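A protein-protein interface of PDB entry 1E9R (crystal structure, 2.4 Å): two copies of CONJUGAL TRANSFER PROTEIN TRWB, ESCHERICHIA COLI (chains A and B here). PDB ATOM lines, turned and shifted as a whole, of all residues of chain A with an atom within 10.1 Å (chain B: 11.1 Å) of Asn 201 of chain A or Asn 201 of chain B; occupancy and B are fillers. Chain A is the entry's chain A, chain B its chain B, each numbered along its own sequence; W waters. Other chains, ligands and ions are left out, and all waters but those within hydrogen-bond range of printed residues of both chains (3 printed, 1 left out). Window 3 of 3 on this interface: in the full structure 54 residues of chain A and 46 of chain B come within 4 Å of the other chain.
OG1 of Thr 208 of chain A is in hydrogen-bond range of OG of Ser 200 of chain B (2.4 Å).
The backbone carbonyl oxygen (O) of Ser 200 of chain A lies within hydrogen-bond range of the side-chain hydroxyl (OG) of Ser 204 of chain A (3.3 Å). The backbone NH of Ala 203 of chain B lies within hydrogen-bond range of the side-chain hydroxyl of Ser 200 of chain B (3.2 Å). N of Glu 202 of chain B lies close to OG of Ser 200 of chain B. O of Lys 205 of chain A is in hydrogen-bond range of OG of Ser 209 of chain A (3.1 Å).
Phe 181 of chain A touches Gly 199 of chain B. CB of Ser 204 of chain A touches CB of Ser 200 of chain B, 3.9 Å away. OE1 of Glu 202 of chain B touches CE of Lys 205 of chain A, at 3.7 Å. Glu 202 of chain B touches Thr 208 of chain A. Thr 208 of chain A touches Ala 203 of chain B. Phe 212 of chain A touches Tyr 149 of chain B (CZ to CE1, 3.7 Å). Leu 196 of chain B touches Phe 212 of chain A (O to CZ, 3.3 Å). Phe 212 of chain A touches Ala 206 of chain B.
Arg 185 of chain A touches none of the printed residues of chain B. Leu 196 of chain A touches none of the printed residues of chain B. No residue of chain B comes within 4 Å of Gly 199 of chain A. No residue of chain B comes within 4 Å of Ser 200 of chain A. Asn 201 of chain A touches just one residue of chain B: Asn 201 (3.7 Å). No residue of chain B comes within 4 Å of Glu 202 of chain A. Printed residues of chain B within 4 Å of Lys 205 of chain A: Glu 202. Printed residues of chain B within 4 Å of Thr 208 of chain A: Ser 200 (2.4 Å), Glu 202 (3.6 Å) and Ala 203 (3.6 Å). Printed residues of chain A within 4 Å of Leu 196 of chain B: Phe 212 (3.3 Å). Ala 203 of chain B touches just one residue of chain A: Thr 208 (3.6 Å). No residue of chain A comes within 4 Å of Ser 204 of chain B. The nearest printed residue of chain A that does not touch Asn 201 of chain B is Ser 204 of chain A (5.8 Å). The nearest printed residue of chain B that does not touch Phe 181 of chain A is Ser 200 of chain B (4.1 Å).
Of the 20 printed residues of chain B, 8 touch a printed residue of chain A. Hydrophobic or aromatic side chains of chain B that line the printed part of chain A: Tyr 149, Leu 196, Ala 203 and Ala 206. Along chain B the printed residues that touch a printed residue of chain A span positions 149 to 206. Printed residues of chain A that touch a printed residue of chain B: Phe 181, Asn 201, Ser 204, Lys 205, Thr 208 and Phe 212. Among the printed residues, 10 pairs touch across the chains. Among the printed residues, no Asp or Glu carboxylate lies within 4 Å of a Lys or Arg side-chain nitrogen of the other chain.
Lys 205 of chain A touches Glu 202 of chain B, but with the chains exchanged Glu 202 of chain A does not touch Lys 205 of chain B (10.2 Å). Thr 208 of chain A touches Ser 200 of chain B, but with the chains exchanged Ser 200 of chain A does not touch Thr 208 of chain B (18.2 Å). Of the 10 pairs that touch across the chains among the printed residues, 1 has its exchanged pair printed and touching as well.
Water W2 lies within hydrogen-bond range of N of Phe 181 of chain A and O of Ala 198 of chain B. Water W3 lies within hydrogen-bond range of the side-chain hydroxyl (OH) of Tyr 149 of chain B (3.0 Å), the side-chain carboxylate (OE2) of Glu 202 of chain B (3.1 Å) and the side-chain hydroxyl (OG) of Ser 209 of chain A (3.5 Å). Water W1 bridges the side-chain amide oxygen of Asn 201 of chain A (3.0 Å) and the side-chain amide nitrogen of Asn 201 of chain B (3.1 Å).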
ATOM      1  N   TYR A 149     -19.126   1.479  -4.413  1.00  0.00           N
ATOM      2  CA  TYR A 149     -18.811   1.146  -3.027  1.00  0.00           C
ATOM      3  C   TYR A 149     -19.264  -0.280  -2.771  1.00  0.00           C
ATOM      4  O   TYR A 149     -18.599  -1.025  -2.066  1.00  0.00           O
ATOM      5  CB  TYR A 149     -19.556   2.074  -2.074  1.00  0.00           C
ATOM      6  CG  TYR A 149     -19.156   3.521  -2.204  1.00  0.00           C
ATOM      7  CD1 TYR A 149     -17.820   3.879  -2.417  1.00  0.00           C
ATOM      8  CD2 TYR A 149     -20.111   4.539  -2.103  1.00  0.00           C
ATOM      9  CE1 TYR A 149     -17.442   5.210  -2.529  1.00  0.00           C
ATOM     10  CE2 TYR A 149     -19.747   5.876  -2.214  1.00  0.00           C
ATOM     11  CZ  TYR A 149     -18.408   6.203  -2.427  1.00  0.00           C
ATOM     12  OH  TYR A 149     -18.031   7.524  -2.549  1.00  0.00           O
ATOM     13  N   PHE A 181     -22.544  -2.944  11.834  1.00  0.00           N
ATOM     14  CA  PHE A 181     -21.576  -2.061  11.211  1.00  0.00           C
ATOM     15  C   PHE A 181     -20.172  -2.329  11.740  1.00  0.00           C
ATOM     16  O   PHE A 181     -19.226  -2.506  10.973  1.00  0.00           O
ATOM     17  CB  PHE A 181     -21.959  -0.620  11.514  1.00  0.00           C
ATOM     18  CG  PHE A 181     -21.720   0.322  10.383  1.00  0.00           C
ATOM     19  CD1 PHE A 181     -22.419   0.177   9.190  1.00  0.00           C
ATOM     20  CD2 PHE A 181     -20.829   1.380  10.520  1.00  0.00           C
ATOM     21  CE1 PHE A 181     -22.239   1.078   8.149  1.00  0.00           C
ATOM     22  CE2 PHE A 181     -20.641   2.288   9.487  1.00  0.00           C
ATOM     23  CZ  PHE A 181     -21.348   2.138   8.296  1.00  0.00           C
ATOM     24  N   ARG A 185     -16.830  -4.030   9.992  1.00  0.00           N
ATOM     25  CA  ARG A 185     -15.588  -3.271  10.028  1.00  0.00           C
ATOM     26  C   ARG A 185     -14.444  -4.167  10.496  1.00  0.00           C
ATOM     27  O   ARG A 185     -13.362  -4.174   9.902  1.00  0.00           O
ATOM     28  CB  ARG A 185     -15.743  -2.098  10.987  1.00  0.00           C
ATOM     29  CG  ARG A 185     -16.500  -0.916  10.431  1.00  0.00           C
ATOM     30  CD  ARG A 185     -15.537   0.033   9.747  1.00  0.00           C
ATOM     31  NE  ARG A 185     -16.170   1.291   9.366  1.00  0.00           N
ATOM     32  CZ  ARG A 185     -16.673   2.179  10.219  1.00  0.00           C
ATOM     33  NH1 ARG A 185     -16.619   1.955  11.525  1.00  0.00           N
ATOM     34  NH2 ARG A 185     -17.230   3.295   9.759  1.00  0.00           N
ATOM     35  N   SER A 195      -9.501   0.490   5.749  1.00  0.00           N
ATOM     36  CA  SER A 195      -9.450   1.928   5.937  1.00  0.00           C
ATOM     37  C   SER A 195     -10.352   2.755   5.032  1.00  0.00           C
ATOM     38  O   SER A 195     -10.769   3.853   5.402  1.00  0.00           O
ATOM     39  CB  SER A 195      -8.009   2.410   5.776  1.00  0.00           C
ATOM     40  OG  SER A 195      -7.167   1.818   6.749  1.00  0.00           O
ATOM     41  N   LEU A 196     -10.648   2.248   3.843  1.00  0.00           N
ATOM     42  CA  LEU A 196     -11.490   2.996   2.921  1.00  0.00           C
ATOM     43  C   LEU A 196     -12.872   3.263   3.479  1.00  0.00           C
ATOM     44  O   LEU A 196     -13.456   4.287   3.189  1.00  0.00           O
ATOM     45  CB  LEU A 196     -11.593   2.276   1.573  1.00  0.00           C
ATOM     46  CG  LEU A 196     -10.285   2.272   0.777  1.00  0.00           C
ATOM     47  CD1 LEU A 196     -10.437   1.442  -0.461  1.00  0.00           C
ATOM     48  CD2 LEU A 196      -9.903   3.692   0.413  1.00  0.00           C
ATOM     49  N   PHE A 197     -13.387   2.358   4.295  1.00  0.00           N
ATOM     50  CA  PHE A 197     -14.713   2.540   4.864  1.00  0.00           C
ATOM     51  C   PHE A 197     -14.706   3.073   6.298  1.00  0.00           C
ATOM     52  O   PHE A 197     -15.683   2.915   7.028  1.00  0.00           O
ATOM     53  CB  PHE A 197     -15.478   1.218   4.810  1.00  0.00           C
ATOM     54  CG  PHE A 197     -16.015   0.884   3.450  1.00  0.00           C
ATOM     55  CD1 PHE A 197     -16.722   1.832   2.716  1.00  0.00           C
ATOM     56  CD2 PHE A 197     -15.834  -0.382   2.908  1.00  0.00           C
ATOM     57  CE1 PHE A 197     -17.240   1.519   1.463  1.00  0.00           C
ATOM     58  CE2 PHE A 197     -16.349  -0.706   1.652  1.00  0.00           C
ATOM     59  CZ  PHE A 197     -17.052   0.243   0.929  1.00  0.00           C
ATOM     60  N   ALA A 198     -13.617   3.718   6.705  1.00  0.00           N
ATOM     61  CA  ALA A 198     -13.536   4.251   8.065  1.00  0.00           C
ATOM     62  C   ALA A 198     -12.792   5.582   8.108  1.00  0.00           C
ATOM     63  O   ALA A 198     -12.109   5.950   7.153  1.00  0.00           O
ATOM     64  CB  ALA A 198     -12.853   3.230   8.997  1.00  0.00           C
ATOM     65  N   GLY A 199     -12.953   6.315   9.206  1.00  0.00           N
ATOM     66  CA  GLY A 199     -12.260   7.584   9.329  1.00  0.00           C
ATOM     67  C   GLY A 199     -13.064   8.870   9.243  1.00  0.00           C
ATOM     68  O   GLY A 199     -12.596   9.915   9.701  1.00  0.00           O
ATOM     69  N   SER A 200     -14.257   8.824   8.655  1.00  0.00           N
ATOM     70  CA  SER A 200     -15.078  10.030   8.552  1.00  0.00           C
ATOM     71  C   SER A 200     -16.528   9.668   8.347  1.00  0.00           C
ATOM     72  O   SER A 200     -16.859   8.498   8.142  1.00  0.00           O
ATOM     73  CB  SER A 200     -14.607  10.907   7.388  1.00  0.00           C
ATOM     74  OG  SER A 200     -14.854  10.287   6.135  1.00  0.00           O
ATOM     75  N   ASN A 201     -17.395  10.672   8.410  1.00  0.00           N
ATOM     76  CA  ASN A 201     -18.810  10.434   8.202  1.00  0.00           C
ATOM     77  C   ASN A 201     -19.011  10.007   6.759  1.00  0.00           C
ATOM     78  O   ASN A 201     -19.855   9.155   6.459  1.00  0.00           O
ATOM     79  CB  ASN A 201     -19.612  11.697   8.484  1.00  0.00           C
ATOM     80  CG  ASN A 201     -19.570  12.088   9.937  1.00  0.00           C
ATOM     81  OD1 ASN A 201     -19.853  11.265  10.820  1.00  0.00           O
ATOM     82  ND2 ASN A 201     -19.229  13.353  10.203  1.00  0.00           N
ATOM     83  N   GLU A 202     -18.225  10.609   5.873  1.00  0.00           N
ATOM     84  CA  GLU A 202     -18.296  10.304   4.454  1.00  0.00           C
ATOM     85  C   GLU A 202     -17.997   8.826   4.220  1.00  0.00           C
ATOM     86  O   GLU A 202     -18.677   8.164   3.431  1.00  0.00           O
ATOM     87  CB  GLU A 202     -17.295  11.166   3.675  1.00  0.00           C
ATOM     88  CG  GLU A 202     -17.287  10.900   2.175  1.00  0.00           C
ATOM     89  CD  GLU A 202     -18.618  11.240   1.500  1.00  0.00           C
ATOM     90  OE1 GLU A 202     -19.491  11.855   2.163  1.00  0.00           O
ATOM     91  OE2 GLU A 202     -18.787  10.893   0.301  1.00  0.00           O
ATOM     92  N   ALA A 203     -16.982   8.312   4.912  1.00  0.00           N
ATOM     93  CA  ALA A 203     -16.593   6.912   4.787  1.00  0.00           C
ATOM     94  C   ALA A 203     -17.695   5.985   5.308  1.00  0.00           C
ATOM     95  O   ALA A 203     -17.977   4.946   4.718  1.00  0.00           O
ATOM     96  CB  ALA A 203     -15.299   6.666   5.542  1.00  0.00           C
ATOM     97  N   SER A 204     -18.315   6.363   6.415  1.00  0.00           N
ATOM     98  CA  SER A 204     -19.385   5.560   6.972  1.00  0.00           C
ATOM     99  C   SER A 204     -20.566   5.567   6.018  1.00  0.00           C
ATOM    100  O   SER A 204     -21.245   4.558   5.851  1.00  0.00           O
ATOM    101  CB  SER A 204     -19.812   6.127   8.319  1.00  0.00           C
ATOM    102  OG  SER A 204     -18.751   6.013   9.240  1.00  0.00           O
ATOM    103  N   LYS A 205     -20.808   6.720   5.402  1.00  0.00           N
ATOM    104  CA  LYS A 205     -21.908   6.872   4.468  1.00  0.00           C
ATOM    105  C   LYS A 205     -21.690   5.948   3.290  1.00  0.00           C
ATOM    106  O   LYS A 205     -22.623   5.297   2.810  1.00  0.00           O
ATOM    107  CB  LYS A 205     -21.986   8.311   3.977  1.00  0.00           C
ATOM    108  CG  LYS A 205     -23.018   8.501   2.903  1.00  0.00           C
ATOM    109  CD  LYS A 205     -23.105   9.934   2.483  1.00  0.00           C
ATOM    110  CE  LYS A 205     -24.058  10.083   1.310  1.00  0.00           C
ATOM    111  NZ  LYS A 205     -24.242  11.522   0.954  1.00  0.00           N
ATOM    112  N   ALA A 206     -20.446   5.900   2.827  1.00  0.00           N
ATOM    113  CA  ALA A 206     -20.076   5.039   1.713  1.00  0.00           C
ATOM    114  C   ALA A 206     -20.369   3.576   2.047  1.00  0.00           C
ATOM    115  O   ALA A 206     -20.934   2.851   1.231  1.00  0.00           O
ATOM    116  CB  ALA A 206     -18.598   5.212   1.394  1.00  0.00           C
ATOM    117  N   LEU A 207     -19.988   3.148   3.250  1.00  0.00           N
ATOM    118  CA  LEU A 207     -20.214   1.769   3.687  1.00  0.00           C
ATOM    119  C   LEU A 207     -21.709   1.484   3.718  1.00  0.00           C
ATOM    120  O   LEU A 207     -22.164   0.465   3.211  1.00  0.00           O
ATOM    121  CB  LEU A 207     -19.615   1.537   5.083  1.00  0.00           C
ATOM    122  CG  LEU A 207     -18.974   0.173   5.389  1.00  0.00           C
ATOM    123  CD1 LEU A 207     -19.053  -0.085   6.877  1.00  0.00           C
ATOM    124  CD2 LEU A 207     -19.678  -0.944   4.641  1.00  0.00           C
ATOM    125  N   THR A 208     -22.469   2.391   4.315  1.00  0.00           N
ATOM    126  CA  THR A 208     -23.916   2.232   4.392  1.00  0.00           C
ATOM    127  C   THR A 208     -24.484   2.061   2.990  1.00  0.00           C
ATOM    128  O   THR A 208     -25.348   1.204   2.762  1.00  0.00           O
ATOM    129  CB  THR A 208     -24.566   3.451   5.036  1.00  0.00           C
ATOM    130  OG1 THR A 208     -24.068   3.601   6.370  1.00  0.00           O
ATOM    131  CG2 THR A 208     -26.080   3.292   5.055  1.00  0.00           C
ATOM    132  N   SER A 209     -23.996   2.877   2.055  1.00  0.00           N
ATOM    133  CA  SER A 209     -24.438   2.818   0.656  1.00  0.00           C
ATOM    134  C   SER A 209     -24.175   1.442   0.067  1.00  0.00           C
ATOM    135  O   SER A 209     -25.045   0.845  -0.575  1.00  0.00           O
ATOM    136  CB  SER A 209     -23.701   3.864  -0.183  1.00  0.00           C
ATOM    137  OG  SER A 209     -24.142   5.163   0.153  1.00  0.00           O
ATOM    138  N   PHE A 212     -26.609  -1.253   1.301  1.00  0.00           N
ATOM    139  CA  PHE A 212     -27.891  -1.180   0.625  1.00  0.00           C
ATOM    140  C   PHE A 212     -27.847  -1.743  -0.782  1.00  0.00           C
ATOM    141  O   PHE A 212     -28.765  -2.435  -1.197  1.00  0.00           O
ATOM    142  CB  PHE A 212     -28.381   0.261   0.585  1.00  0.00           C
ATOM    143  CG  PHE A 212     -29.040   0.691   1.843  1.00  0.00           C
ATOM    144  CD1 PHE A 212     -30.124  -0.027   2.343  1.00  0.00           C
ATOM    145  CD2 PHE A 212     -28.581   1.807   2.541  1.00  0.00           C
ATOM    146  CE1 PHE A 212     -30.742   0.354   3.514  1.00  0.00           C
ATOM    147  CE2 PHE A 212     -29.193   2.200   3.716  1.00  0.00           C
ATOM    148  CZ  PHE A 212     -30.278   1.472   4.208  1.00  0.00           C
ATOM    149  N   GLU B 145     -35.608   6.198  -4.351  1.00  0.00           N
ATOM    150  CA  GLU B 145     -34.612   5.692  -3.414  1.00  0.00           C
ATOM    151  C   GLU B 145     -35.298   5.566  -2.050  1.00  0.00           C
ATOM    152  O   GLU B 145     -35.178   4.543  -1.373  1.00  0.00           O
ATOM    153  CB  GLU B 145     -33.417   6.648  -3.318  1.00  0.00           C
ATOM    154  CG  GLU B 145     -32.303   6.153  -2.396  1.00  0.00           C
ATOM    155  CD  GLU B 145     -31.349   7.266  -1.934  1.00  0.00           C
ATOM    156  OE1 GLU B 145     -31.510   8.422  -2.401  1.00  0.00           O
ATOM    157  OE2 GLU B 145     -30.442   6.984  -1.103  1.00  0.00           O
ATOM    158  N   TYR B 149     -36.321   2.277   0.533  1.00  0.00           N
ATOM    159  CA  TYR B 149     -36.075   2.077   1.957  1.00  0.00           C
ATOM    160  C   TYR B 149     -37.409   1.748   2.614  1.00  0.00           C
ATOM    161  O   TYR B 149     -37.470   0.940   3.545  1.00  0.00           O
ATOM    162  CB  TYR B 149     -35.495   3.351   2.579  1.00  0.00           C
ATOM    163  CG  TYR B 149     -34.138   3.751   2.041  1.00  0.00           C
ATOM    164  CD1 TYR B 149     -33.158   2.798   1.789  1.00  0.00           C
ATOM    165  CD2 TYR B 149     -33.833   5.088   1.786  1.00  0.00           C
ATOM    166  CE1 TYR B 149     -31.904   3.161   1.296  1.00  0.00           C
ATOM    167  CE2 TYR B 149     -32.584   5.463   1.294  1.00  0.00           C
ATOM    168  CZ  TYR B 149     -31.624   4.493   1.050  1.00  0.00           C
ATOM    169  OH  TYR B 149     -30.389   4.852   0.553  1.00  0.00           O
ATOM    170  N   PHE B 181     -37.876   5.585  17.242  1.00  0.00           N
ATOM    171  CA  PHE B 181     -36.776   5.122  16.414  1.00  0.00           C
ATOM    172  C   PHE B 181     -36.117   3.910  17.032  1.00  0.00           C
ATOM    173  O   PHE B 181     -35.879   2.907  16.362  1.00  0.00           O
ATOM    174  CB  PHE B 181     -35.735   6.221  16.299  1.00  0.00           C
ATOM    175  CG  PHE B 181     -35.110   6.332  14.944  1.00  0.00           C
ATOM    176  CD1 PHE B 181     -35.870   6.718  13.841  1.00  0.00           C
ATOM    177  CD2 PHE B 181     -33.746   6.134  14.780  1.00  0.00           C
ATOM    178  CE1 PHE B 181     -35.280   6.917  12.599  1.00  0.00           C
ATOM    179  CE2 PHE B 181     -33.145   6.331  13.537  1.00  0.00           C
ATOM    180  CZ  PHE B 181     -33.918   6.726  12.446  1.00  0.00           C
ATOM    181  N   ARG B 185     -36.057  -0.102  15.912  1.00  0.00           N
ATOM    182  CA  ARG B 185     -34.773  -0.778  15.745  1.00  0.00           C
ATOM    183  C   ARG B 185     -34.792  -2.123  16.469  1.00  0.00           C
ATOM    184  O   ARG B 185     -34.388  -3.142  15.921  1.00  0.00           O
ATOM    185  CB  ARG B 185     -33.650   0.086  16.318  1.00  0.00           C
ATOM    186  CG  ARG B 185     -33.267   1.296  15.480  1.00  0.00           C
ATOM    187  CD  ARG B 185     -32.048   0.977  14.643  1.00  0.00           C
ATOM    188  NE  ARG B 185     -31.566   2.118  13.870  1.00  0.00           N
ATOM    189  CZ  ARG B 185     -31.158   3.266  14.397  1.00  0.00           C
ATOM    190  NH1 ARG B 185     -31.186   3.438  15.707  1.00  0.00           N
ATOM    191  NH2 ARG B 185     -30.729   4.243  13.611  1.00  0.00           N
ATOM    192  N   SER B 195     -29.528  -4.545  10.744  1.00  0.00           N
ATOM    193  CA  SER B 195     -28.350  -3.709  10.587  1.00  0.00           C
ATOM    194  C   SER B 195     -28.350  -2.722   9.424  1.00  0.00           C
ATOM    195  O   SER B 195     -27.532  -1.805   9.411  1.00  0.00           O
ATOM    196  CB  SER B 195     -27.109  -4.598  10.492  1.00  0.00           C
ATOM    197  OG  SER B 195     -27.014  -5.440  11.624  1.00  0.00           O
ATOM    198  N   LEU B 196     -29.237  -2.895   8.445  1.00  0.00           N
ATOM    199  CA  LEU B 196     -29.264  -1.975   7.304  1.00  0.00           C
ATOM    200  C   LEU B 196     -29.673  -0.571   7.715  1.00  0.00           C
ATOM    201  O   LEU B 196     -29.210   0.404   7.134  1.00  0.00           O
ATOM    202  CB  LEU B 196     -30.201  -2.483   6.203  1.00  0.00           C
ATOM    203  CG  LEU B 196     -29.590  -3.583   5.332  1.00  0.00           C
ATOM    204  CD1 LEU B 196     -30.611  -4.119   4.341  1.00  0.00           C
ATOM    205  CD2 LEU B 196     -28.383  -3.020   4.604  1.00  0.00           C
ATOM    206  N   PHE B 197     -30.525  -0.465   8.729  1.00  0.00           N
ATOM    207  CA  PHE B 197     -30.979   0.842   9.197  1.00  0.00           C
ATOM    208  C   PHE B 197     -30.242   1.354  10.436  1.00  0.00           C
ATOM    209  O   PHE B 197     -30.756   2.217  11.153  1.00  0.00           O
ATOM    210  CB  PHE B 197     -32.485   0.803   9.486  1.00  0.00           C
ATOM    211  CG  PHE B 197     -33.341   0.796   8.252  1.00  0.00           C
ATOM    212  CD1 PHE B 197     -33.117   1.717   7.230  1.00  0.00           C
ATOM    213  CD2 PHE B 197     -34.367  -0.133   8.104  1.00  0.00           C
ATOM    214  CE1 PHE B 197     -33.901   1.714   6.069  1.00  0.00           C
ATOM    215  CE2 PHE B 197     -35.157  -0.144   6.947  1.00  0.00           C
ATOM    216  CZ  PHE B 197     -34.920   0.787   5.927  1.00  0.00           C
ATOM    217  N   ALA B 198     -29.039   0.844  10.688  1.00  0.00           N
ATOM    218  CA  ALA B 198     -28.277   1.273  11.857  1.00  0.00           C
ATOM    219  C   ALA B 198     -26.777   1.334  11.598  1.00  0.00           C
ATOM    220  O   ALA B 198     -26.269   0.717  10.656  1.00  0.00           O
ATOM    221  CB  ALA B 198     -28.569   0.335  13.024  1.00  0.00           C
ATOM    222  N   GLY B 199     -26.075   2.107  12.424  1.00  0.00           N
ATOM    223  CA  GLY B 199     -24.634   2.197  12.285  1.00  0.00           C
ATOM    224  C   GLY B 199     -24.016   3.491  11.795  1.00  0.00           C
ATOM    225  O   GLY B 199     -22.822   3.714  11.990  1.00  0.00           O
ATOM    226  N   SER B 200     -24.792   4.343  11.135  1.00  0.00           N
ATOM    227  CA  SER B 200     -24.248   5.609  10.649  1.00  0.00           C
ATOM    228  C   SER B 200     -25.377   6.593  10.457  1.00  0.00           C
ATOM    229  O   SER B 200     -26.548   6.215  10.527  1.00  0.00           O
ATOM    230  CB  SER B 200     -23.514   5.415   9.324  1.00  0.00           C
ATOM    231  OG  SER B 200     -24.419   5.038   8.304  1.00  0.00           O
ATOM    232  N   ASN B 201     -25.029   7.853  10.225  1.00  0.00           N
ATOM    233  CA  ASN B 201     -26.043   8.875  10.020  1.00  0.00           C
ATOM    234  C   ASN B 201     -26.815   8.558   8.754  1.00  0.00           C
ATOM    235  O   ASN B 201     -28.023   8.785   8.680  1.00  0.00           O
ATOM    236  CB  ASN B 201     -25.402  10.263   9.913  1.00  0.00           C
ATOM    237  CG  ASN B 201     -24.780  10.714  11.221  1.00  0.00           C
ATOM    238  OD1 ASN B 201     -25.438  10.694  12.265  1.00  0.00           O
ATOM    239  ND2 ASN B 201     -23.510  11.131  11.172  1.00  0.00           N
ATOM    240  N   GLU B 202     -26.107   8.020   7.765  1.00  0.00           N
ATOM    241  CA  GLU B 202     -26.715   7.645   6.492  1.00  0.00           C
ATOM    242  C   GLU B 202     -27.804   6.583   6.694  1.00  0.00           C
ATOM    243  O   GLU B 202     -28.907   6.674   6.138  1.00  0.00           O
ATOM    244  CB  GLU B 202     -25.647   7.120   5.538  1.00  0.00           C
ATOM    245  CG  GLU B 202     -26.199   6.746   4.182  1.00  0.00           C
ATOM    246  CD  GLU B 202     -26.824   7.923   3.452  1.00  0.00           C
ATOM    247  OE1 GLU B 202     -26.582   9.086   3.849  1.00  0.00           O
ATOM    248  OE2 GLU B 202     -27.556   7.682   2.468  1.00  0.00           O
ATOM    249  N   ALA B 203     -27.487   5.578   7.498  1.00  0.00           N
ATOM    250  CA  ALA B 203     -28.435   4.521   7.797  1.00  0.00           C
ATOM    251  C   ALA B 203     -29.666   5.087   8.519  1.00  0.00           C
ATOM    252  O   ALA B 203     -30.796   4.698   8.226  1.00  0.00           O
ATOM    253  CB  ALA B 203     -27.757   3.449   8.651  1.00  0.00           C
ATOM    254  N   SER B 204     -29.433   6.005   9.459  1.00  0.00           N
ATOM    255  CA  SER B 204     -30.509   6.636  10.225  1.00  0.00           C
ATOM    256  C   SER B 204     -31.377   7.463   9.304  1.00  0.00           C
ATOM    257  O   SER B 204     -32.599   7.498   9.447  1.00  0.00           O
ATOM    258  CB  SER B 204     -29.944   7.553  11.315  1.00  0.00           C
ATOM    259  OG  SER B 204     -29.368   6.804  12.372  1.00  0.00           O
ATOM    260  N   LYS B 205     -30.725   8.144   8.372  1.00  0.00           N
ATOM    261  CA  LYS B 205     -31.415   8.974   7.407  1.00  0.00           C
ATOM    262  C   LYS B 205     -32.303   8.089   6.540  1.00  0.00           C
ATOM    263  O   LYS B 205     -33.454   8.434   6.229  1.00  0.00           O
ATOM    264  CB  LYS B 205     -30.398   9.698   6.543  1.00  0.00           C
ATOM    265  CG  LYS B 205     -31.023  10.425   5.391  1.00  0.00           C
ATOM    266  CD  LYS B 205     -29.987  11.195   4.609  1.00  0.00           C
ATOM    267  CE  LYS B 205     -30.630  11.857   3.395  1.00  0.00           C
ATOM    268  NZ  LYS B 205     -29.641  12.610   2.577  1.00  0.00           N
ATOM    269  N   ALA B 206     -31.758   6.939   6.155  1.00  0.00           N
ATOM    270  CA  ALA B 206     -32.493   5.981   5.347  1.00  0.00           C
ATOM    271  C   ALA B 206     -33.747   5.529   6.097  1.00  0.00           C
ATOM    272  O   ALA B 206     -34.835   5.509   5.528  1.00  0.00           O
ATOM    273  CB  ALA B 206     -31.610   4.796   5.025  1.00  0.00           C
ATOM    274  N   LEU B 207     -33.601   5.187   7.378  1.00  0.00           N
ATOM    275  CA  LEU B 207     -34.742   4.750   8.190  1.00  0.00           C
ATOM    276  C   LEU B 207     -35.783   5.861   8.239  1.00  0.00           C
ATOM    277  O   LEU B 207     -36.970   5.615   8.028  1.00  0.00           O
ATOM    278  CB  LEU B 207     -34.311   4.425   9.625  1.00  0.00           C
ATOM    279  CG  LEU B 207     -35.043   3.311  10.393  1.00  0.00           C
ATOM    280  CD1 LEU B 207     -34.970   3.582  11.890  1.00  0.00           C
ATOM    281  CD2 LEU B 207     -36.482   3.229   9.959  1.00  0.00           C
ATOM    282  N   THR B 208     -35.329   7.081   8.529  1.00  0.00           N
ATOM    283  CA  THR B 208     -36.215   8.238   8.604  1.00  0.00           C
ATOM    284  C   THR B 208     -36.992   8.379   7.311  1.00  0.00           C
ATOM    285  O   THR B 208     -38.195   8.645   7.333  1.00  0.00           O
ATOM    286  CB  THR B 208     -35.434   9.549   8.827  1.00  0.00           C
ATOM    287  OG1 THR B 208     -34.940   9.595  10.165  1.00  0.00           O
ATOM    288  CG2 THR B 208     -36.327  10.735   8.615  1.00  0.00           C
ATOM    289  N   SER B 209     -36.299   8.210   6.186  1.00  0.00           N
ATOM    290  CA  SER B 209     -36.940   8.316   4.877  1.00  0.00           C
ATOM    291  C   SER B 209     -38.027   7.268   4.687  1.00  0.00           C
ATOM    292  O   SER B 209     -39.115   7.568   4.192  1.00  0.00           O
ATOM    293  CB  SER B 209     -35.903   8.179   3.775  1.00  0.00           C
ATOM    294  OG  SER B 209     -35.114   9.343   3.730  1.00  0.00           O
ATOM    295  N   ALA B 210     -37.721   6.038   5.084  1.00  0.00           N
ATOM    296  CA  ALA B 210     -38.665   4.941   4.980  1.00  0.00           C
ATOM    297  C   ALA B 210     -39.927   5.300   5.764  1.00  0.00           C
ATOM    298  O   ALA B 210     -41.030   5.199   5.245  1.00  0.00           O
ATOM    299  CB  ALA B 210     -38.030   3.661   5.532  1.00  0.00           C
HETATM  300  O   HOH W   1     -21.576   8.830  10.325  1.00  0.00           O
HETATM  301  O   HOH W   2     -25.374  -1.998  12.266  1.00  0.00           O
HETATM  302  O   HOH W   3     -27.444   4.795   1.219  1.00  0.00           O
